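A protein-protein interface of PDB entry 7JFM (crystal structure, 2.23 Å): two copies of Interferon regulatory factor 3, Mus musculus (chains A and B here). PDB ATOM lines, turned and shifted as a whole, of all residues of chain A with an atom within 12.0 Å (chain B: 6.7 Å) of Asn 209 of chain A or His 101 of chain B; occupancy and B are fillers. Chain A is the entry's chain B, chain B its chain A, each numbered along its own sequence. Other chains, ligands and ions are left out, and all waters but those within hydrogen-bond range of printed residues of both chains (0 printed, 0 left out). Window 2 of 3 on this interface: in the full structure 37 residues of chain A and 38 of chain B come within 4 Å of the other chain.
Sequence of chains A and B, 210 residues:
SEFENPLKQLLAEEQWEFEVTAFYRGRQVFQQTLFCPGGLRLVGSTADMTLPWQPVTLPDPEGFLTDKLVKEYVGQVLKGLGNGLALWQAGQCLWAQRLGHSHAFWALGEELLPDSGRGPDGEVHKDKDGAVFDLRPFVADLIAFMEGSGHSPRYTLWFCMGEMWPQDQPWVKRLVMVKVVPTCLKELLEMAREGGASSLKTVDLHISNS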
ATOM      1  N   ASP A 204     -22.995  15.358  -4.599  1.00  0.00           N
ATOM      2  CA  ASP A 204     -24.430  15.503  -4.832  1.00  0.00           C
ATOM      3  C   ASP A 204     -24.653  16.920  -5.355  1.00  0.00           C
ATOM      4  O   ASP A 204     -24.896  17.853  -4.587  1.00  0.00           O
ATOM      5  CB  ASP A 204     -25.230  15.234  -3.559  1.00  0.00           C
ATOM      6  CG  ASP A 204     -26.725  15.184  -3.808  1.00  0.00           C
ATOM      7  OD1 ASP A 204     -27.135  15.163  -4.988  1.00  0.00           O
ATOM      8  OD2 ASP A 204     -27.491  15.167  -2.821  1.00  0.00           O
ATOM      9  N   LEU A 205     -24.566  17.072  -6.673  1.00  0.00           N
ATOM     10  CA  LEU A 205     -24.650  18.384  -7.305  1.00  0.00           C
ATOM     11  C   LEU A 205     -26.074  18.915  -7.200  1.00  0.00           C
ATOM     12  O   LEU A 205     -27.000  18.350  -7.791  1.00  0.00           O
ATOM     13  CB  LEU A 205     -24.203  18.290  -8.760  1.00  0.00           C
ATOM     14  CG  LEU A 205     -23.384  19.467  -9.289  1.00  0.00           C
ATOM     15  CD1 LEU A 205     -22.209  19.737  -8.363  1.00  0.00           C
ATOM     16  CD2 LEU A 205     -22.899  19.184 -10.700  1.00  0.00           C
ATOM     17  N   HIS A 206     -26.254  20.003  -6.449  1.00  0.00           N
ATOM     18  CA  HIS A 206     -27.567  20.626  -6.285  1.00  0.00           C
ATOM     19  C   HIS A 206     -27.764  21.660  -7.391  1.00  0.00           C
ATOM     20  O   HIS A 206     -27.663  22.873  -7.188  1.00  0.00           O
ATOM     21  CB  HIS A 206     -27.702  21.243  -4.899  1.00  0.00           C
ATOM     22  CG  HIS A 206     -28.400  20.361  -3.912  1.00  0.00           C
ATOM     23  ND1 HIS A 206     -29.769  20.358  -3.755  1.00  0.00           N
ATOM     24  CD2 HIS A 206     -27.917  19.454  -3.029  1.00  0.00           C
ATOM     25  CE1 HIS A 206     -30.101  19.486  -2.820  1.00  0.00           C
ATOM     26  NE2 HIS A 206     -28.996  18.924  -2.364  1.00  0.00           N
ATOM     27  N   ILE A 207     -28.052  21.158  -8.590  1.00  0.00           N
ATOM     28  CA  ILE A 207     -28.355  21.989  -9.747  1.00  0.00           C
ATOM     29  C   ILE A 207     -29.666  21.506 -10.353  1.00  0.00           C
ATOM     30  O   ILE A 207     -29.895  20.298 -10.480  1.00  0.00           O
ATOM     31  CB  ILE A 207     -27.218  21.961 -10.793  1.00  0.00           C
ATOM     32  CG1 ILE A 207     -26.960  20.536 -11.287  1.00  0.00           C
ATOM     33  CG2 ILE A 207     -25.944  22.554 -10.213  1.00  0.00           C
ATOM     34  CD1 ILE A 207     -25.968  20.455 -12.425  1.00  0.00           C
ATOM     35  N   SER A 208     -30.530  22.452 -10.712  1.00  0.00           N
ATOM     36  CA  SER A 208     -31.826  22.149 -11.310  1.00  0.00           C
ATOM     37  C   SER A 208     -32.472  23.460 -11.737  1.00  0.00           C
ATOM     38  O   SER A 208     -31.993  24.548 -11.408  1.00  0.00           O
ATOM     39  CB  SER A 208     -32.739  21.389 -10.342  1.00  0.00           C
ATOM     40  OG  SER A 208     -32.985  22.146  -9.171  1.00  0.00           O
ATOM     41  N   ASN A 209     -33.575  23.337 -12.478  1.00  0.00           N
ATOM     42  CA  ASN A 209     -34.336  24.519 -12.872  1.00  0.00           C
ATOM     43  C   ASN A 209     -35.133  25.073 -11.699  1.00  0.00           C
ATOM     44  O   ASN A 209     -35.089  26.277 -11.417  1.00  0.00           O
ATOM     45  CB  ASN A 209     -35.263  24.181 -14.041  1.00  0.00           C
ATOM     46  CG  ASN A 209     -34.545  24.187 -15.376  1.00  0.00           C
ATOM     47  OD1 ASN A 209     -33.317  24.220 -15.431  1.00  0.00           O
ATOM     48  ND2 ASN A 209     -35.311  24.159 -16.459  1.00  0.00           N
ATOM     49  N   SER A 210     -35.866  24.210 -11.002  1.00  0.00           N
ATOM     50  CA  SER A 210     -36.660  24.628  -9.853  1.00  0.00           C
ATOM     51  C   SER A 210     -35.833  24.582  -8.572  1.00  0.00           C
ATOM     52  O   SER A 210     -34.725  25.117  -8.515  1.00  0.00           O
ATOM     53  CB  SER A 210     -37.904  23.749  -9.710  1.00  0.00           C
ATOM     54  OG  SER A 210     -38.726  23.838 -10.861  1.00  0.00           O
ATOM     55  OXT SER A 210     -36.254  24.013  -7.566  1.00  0.00           O
ATOM     56  N   LYS B  79     -20.515  26.573 -14.598  1.00  0.00           N
ATOM     57  CA  LYS B  79     -21.506  26.706 -15.661  1.00  0.00           C
ATOM     58  C   LYS B  79     -22.879  27.032 -15.089  1.00  0.00           C
ATOM     59  O   LYS B  79     -23.621  27.845 -15.654  1.00  0.00           O
ATOM     60  CB  LYS B  79     -21.571  25.424 -16.492  1.00  0.00           C
ATOM     61  CG  LYS B  79     -20.397  25.211 -17.433  1.00  0.00           C
ATOM     62  CD  LYS B  79     -20.460  23.828 -18.068  1.00  0.00           C
ATOM     63  CE  LYS B  79     -19.289  23.586 -19.006  1.00  0.00           C
ATOM     64  NZ  LYS B  79     -19.342  24.466 -20.205  1.00  0.00           N
ATOM     65  N   GLY B  80     -23.233  26.411 -13.964  1.00  0.00           N
ATOM     66  CA  GLY B  80     -24.516  26.652 -13.330  1.00  0.00           C
ATOM     67  C   GLY B  80     -24.676  28.032 -12.729  1.00  0.00           C
ATOM     68  O   GLY B  80     -25.776  28.364 -12.275  1.00  0.00           O
ATOM     69  N   LEU B  81     -23.610  28.837 -12.709  1.00  0.00           N
ATOM     70  CA  LEU B  81     -23.730  30.199 -12.201  1.00  0.00           C
ATOM     71  C   LEU B  81     -24.613  31.055 -13.098  1.00  0.00           C
ATOM     72  O   LEU B  81     -25.309  31.950 -12.605  1.00  0.00           O
ATOM     73  CB  LEU B  81     -22.346  30.831 -12.057  1.00  0.00           C
ATOM     74  CG  LEU B  81     -21.446  30.181 -11.008  1.00  0.00           C
ATOM     75  CD1 LEU B  81     -20.148  30.959 -10.848  1.00  0.00           C
ATOM     76  CD2 LEU B  81     -22.179  30.077  -9.685  1.00  0.00           C
ATOM     77  N   GLY B  82     -24.603  30.795 -14.403  1.00  0.00           N
ATOM     78  CA  GLY B  82     -25.445  31.555 -15.313  1.00  0.00           C
ATOM     79  C   GLY B  82     -25.068  33.020 -15.307  1.00  0.00           C
ATOM     80  O   GLY B  82     -23.893  33.386 -15.421  1.00  0.00           O
ATOM     81  N   ARG B  98     -29.189  34.217  -6.697  1.00  0.00           N
ATOM     82  CA  ARG B  98     -28.603  33.380  -7.734  1.00  0.00           C
ATOM     83  C   ARG B  98     -29.415  33.520  -9.016  1.00  0.00           C
ATOM     84  O   ARG B  98     -30.636  33.334  -9.012  1.00  0.00           O
ATOM     85  CB  ARG B  98     -28.540  31.916  -7.292  1.00  0.00           C
ATOM     86  CG  ARG B  98     -29.846  31.343  -6.769  1.00  0.00           C
ATOM     87  CD  ARG B  98     -29.964  29.865  -7.108  1.00  0.00           C
ATOM     88  NE  ARG B  98     -31.175  29.270  -6.552  1.00  0.00           N
ATOM     89  CZ  ARG B  98     -31.691  28.112  -6.953  1.00  0.00           C
ATOM     90  NH1 ARG B  98     -31.105  27.423  -7.923  1.00  0.00           N
ATOM     91  NH2 ARG B  98     -32.797  27.648  -6.390  1.00  0.00           N
ATOM     92  N   LEU B  99     -28.734  33.866 -10.105  1.00  0.00           N
ATOM     93  CA  LEU B  99     -29.370  34.045 -11.401  1.00  0.00           C
ATOM     94  C   LEU B  99     -29.200  32.837 -12.312  1.00  0.00           C
ATOM     95  O   LEU B  99     -29.662  32.871 -13.458  1.00  0.00           O
ATOM     96  CB  LEU B  99     -28.816  35.297 -12.089  1.00  0.00           C
ATOM     97  CG  LEU B  99     -28.962  36.605 -11.309  1.00  0.00           C
ATOM     98  CD1 LEU B  99     -28.154  37.715 -11.961  1.00  0.00           C
ATOM     99  CD2 LEU B  99     -30.428  37.002 -11.200  1.00  0.00           C
ATOM    100  N   GLY B 100     -28.554  31.777 -11.835  1.00  0.00           N
ATOM    101  CA  GLY B 100     -28.348  30.587 -12.635  1.00  0.00           C
ATOM    102  C   GLY B 100     -29.049  29.363 -12.084  1.00  0.00           C
ATOM    103  O   GLY B 100     -29.944  29.478 -11.241  1.00  0.00           O
ATOM    104  N   HIS B 101     -28.647  28.181 -12.551  1.00  0.00           N
ATOM    105  CA  HIS B 101     -29.283  26.937 -12.135  1.00  0.00           C
ATOM    106  C   HIS B 101     -28.669  26.344 -10.875  1.00  0.00           C
ATOM    107  O   HIS B 101     -29.362  25.638 -10.134  1.00  0.00           O
ATOM    108  CB  HIS B 101     -29.210  25.907 -13.266  1.00  0.00           C
ATOM    109  CG  HIS B 101     -30.054  26.253 -14.452  1.00  0.00           C
ATOM    110  ND1 HIS B 101     -29.708  25.902 -15.739  1.00  0.00           N
ATOM    111  CD2 HIS B 101     -31.231  26.914 -14.546  1.00  0.00           C
ATOM    112  CE1 HIS B 101     -30.635  26.334 -16.575  1.00  0.00           C
ATOM    113  NE2 HIS B 101     -31.570  26.952 -15.878  1.00  0.00           N
ATOM    114  N   SER B 102     -27.392  26.609 -10.615  1.00  0.00           N
ATOM    115  CA  SER B 102     -26.724  26.032  -9.457  1.00  0.00           C
ATOM    116  C   SER B 102     -27.242  26.672  -8.176  1.00  0.00           C
ATOM    117  O   SER B 102     -27.169  27.896  -8.010  1.00  0.00           O
ATOM    118  CB  SER B 102     -25.212  26.212  -9.574  1.00  0.00           C
ATOM    119  OG  SER B 102     -24.863  27.584  -9.622  1.00  0.00           O
ATOM    120  N   HIS B 103     -27.769  25.849  -7.273  1.00  0.00           N
ATOM    121  CA  HIS B 103     -28.215  26.340  -5.980  1.00  0.00           C
ATOM    122  C   HIS B 103     -27.021  26.802  -5.148  1.00  0.00           C
ATOM    123  O   HIS B 103     -25.868  26.456  -5.418  1.00  0.00           O
ATOM    124  CB  HIS B 103     -28.992  25.257  -5.230  1.00  0.00           C
ATOM    125  CG  HIS B 103     -30.253  24.828  -5.916  1.00  0.00           C
ATOM    126  ND1 HIS B 103     -31.501  25.012  -5.362  1.00  0.00           N
ATOM    127  CD2 HIS B 103     -30.457  24.222  -7.110  1.00  0.00           C
ATOM    128  CE1 HIS B 103     -32.420  24.537  -6.184  1.00  0.00           C
ATOM    129  NE2 HIS B 103     -31.812  24.053  -7.252  1.00  0.00           N
ATOM    130  N   ALA B 104     -27.313  27.597  -4.121  1.00  0.00           N
ATOM    131  CA  ALA B 104     -26.267  28.146  -3.271  1.00  0.00           C
ATOM    132  C   ALA B 104     -26.775  28.249  -1.842  1.00  0.00           C
ATOM    133  O   ALA B 104     -27.914  28.662  -1.607  1.00  0.00           O
ATOM    134  CB  ALA B 104     -25.805  29.518  -3.770  1.00  0.00           C
ATOM    135  N   LYS B 126     -33.804  32.828  -5.196  1.00  0.00           N
ATOM    136  CA  LYS B 126     -33.872  33.155  -6.615  1.00  0.00           C
ATOM    137  C   LYS B 126     -34.519  34.511  -6.852  1.00  0.00           C
ATOM    138  O   LYS B 126     -34.279  35.126  -7.896  1.00  0.00           O
ATOM    139  CB  LYS B 126     -34.636  32.067  -7.374  1.00  0.00           C
ATOM    140  CG  LYS B 126     -33.885  30.752  -7.477  1.00  0.00           C
ATOM    141  CD  LYS B 126     -34.622  29.734  -8.333  1.00  0.00           C
ATOM    142  CE  LYS B 126     -35.817  29.145  -7.603  1.00  0.00           C
ATOM    143  NZ  LYS B 126     -36.442  28.040  -8.382  1.00  0.00           N
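The backbone carbonyl oxygen (O) of Gly 80 of chain B lies within hydrogen-bond range of the backbone NH (N) of His 101 of chain B (2.9 Å).
The backbone carbonyl oxygen of Gly 80 of chain B is in hydrogen-bond range of the backbone NH of Ser 102 of chain B.
The guanidinium group (NH1) of Arg 98 of chain B is in hydrogen-bond range of the backbone carbonyl oxygen (O) of His 101 of chain B (3.3 Å).
NH2 of Arg 98 of chain B lies within hydrogen-bond range of ND1 of His 103 of chain B, at 3.1 Å.
NH2 of Arg 98 of chain B lies within salt-bridge range of O of Ser 210 of chain A (3.8 Å).
O of His 101 of chain B sits at hydrogen-bond distance from N of Ser 208 of chain A (3.4 Å).
A ring nitrogen (NE2) of His 101 of chain B is in hydrogen-bond range of the side-chain amide oxygen (OD1) of Asn 209 of chain A, at 3.3 Å.
The backbone NH (N) of His 103 of chain B sits at hydrogen-bond distance from the backbone carbonyl oxygen (O) of His 206 of chain A (3.0 Å).
NE2 of His 103 of chain B sits at hydrogen-bond distance from OG of Ser 208 of chain A (2.9 Å).
The chain-end carboxylate (O) of Ser 210 of chain A sits close to a ring nitrogen (NE2) of His 103 of chain B (3.3 Å).
O of Ser 210 of chain A lies within salt-bridge range of NZ of Lys 126 of chain B (3.4 Å).
Printed residues of chain B within 4 Å of Ile 207 of chain A: His 101 (3.8 Å) and Ser 102 (3.6 Å).
Of the printed residues of chain B, Ser 208 of chain A touches His 101 and His 103.
Asn 209 of chain A touches just these residues of chain B: His 101 and Lys 126.
Of the printed residues of chain B, Ser 210 of chain A touches Arg 98 (3.8 Å), His 103 (3.3 Å) and Lys 126 (3.4 Å).
Printed residues of chain A within 4 Å of Arg 98 of chain B: Ser 210.
No residue of chain A comes within 4 Å of Gly 100 of chain B.
Of chain A, only Ile 207 (3.8 Å), Ser 208 (3.1 Å) and Asn 209 (3.3 Å) come within 4 Å of His 101 of chain B.
Ser 102 of chain B touches just these residues of chain A: His 206 (3.9 Å) and Ile 207 (3.6 Å).
The nearest residue of chain B that does not touch Asn 209 of chain A is Arg 98 of chain B (5.4 Å).
The nearest printed residue of chain B that does not touch Ser 208 of chain A is Arg 98 of chain B (4.6 Å).
No position is printed for both chains.
Among the printed residues, merely in contact across the chains: His 206 of chain A with Ser 102 of chain B, Ile 207 of chain A with His 101 of chain B, Ile 207 of chain A with Ser 102 of chain B and Asn 209 of chain A with Lys 126 of chain B.
Printed residues of chain A that touch a printed residue of chain B: His 206, Ile 207, Ser 208, Asn 209 and Ser 210.
Of the 12 printed residues of chain B, 5 touch a printed residue of chain A.
Printed residues of chain B that touch a printed residue of chain A: Arg 98, His 101, Ser 102, His 103 and Lys 126.
Hydrophobic or aromatic side chains of chain B within 4 Å of the printed part of chain A: His 101 and His 103.
Along chain B the printed residues that touch a printed residue of chain A span positions 98 to 126.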
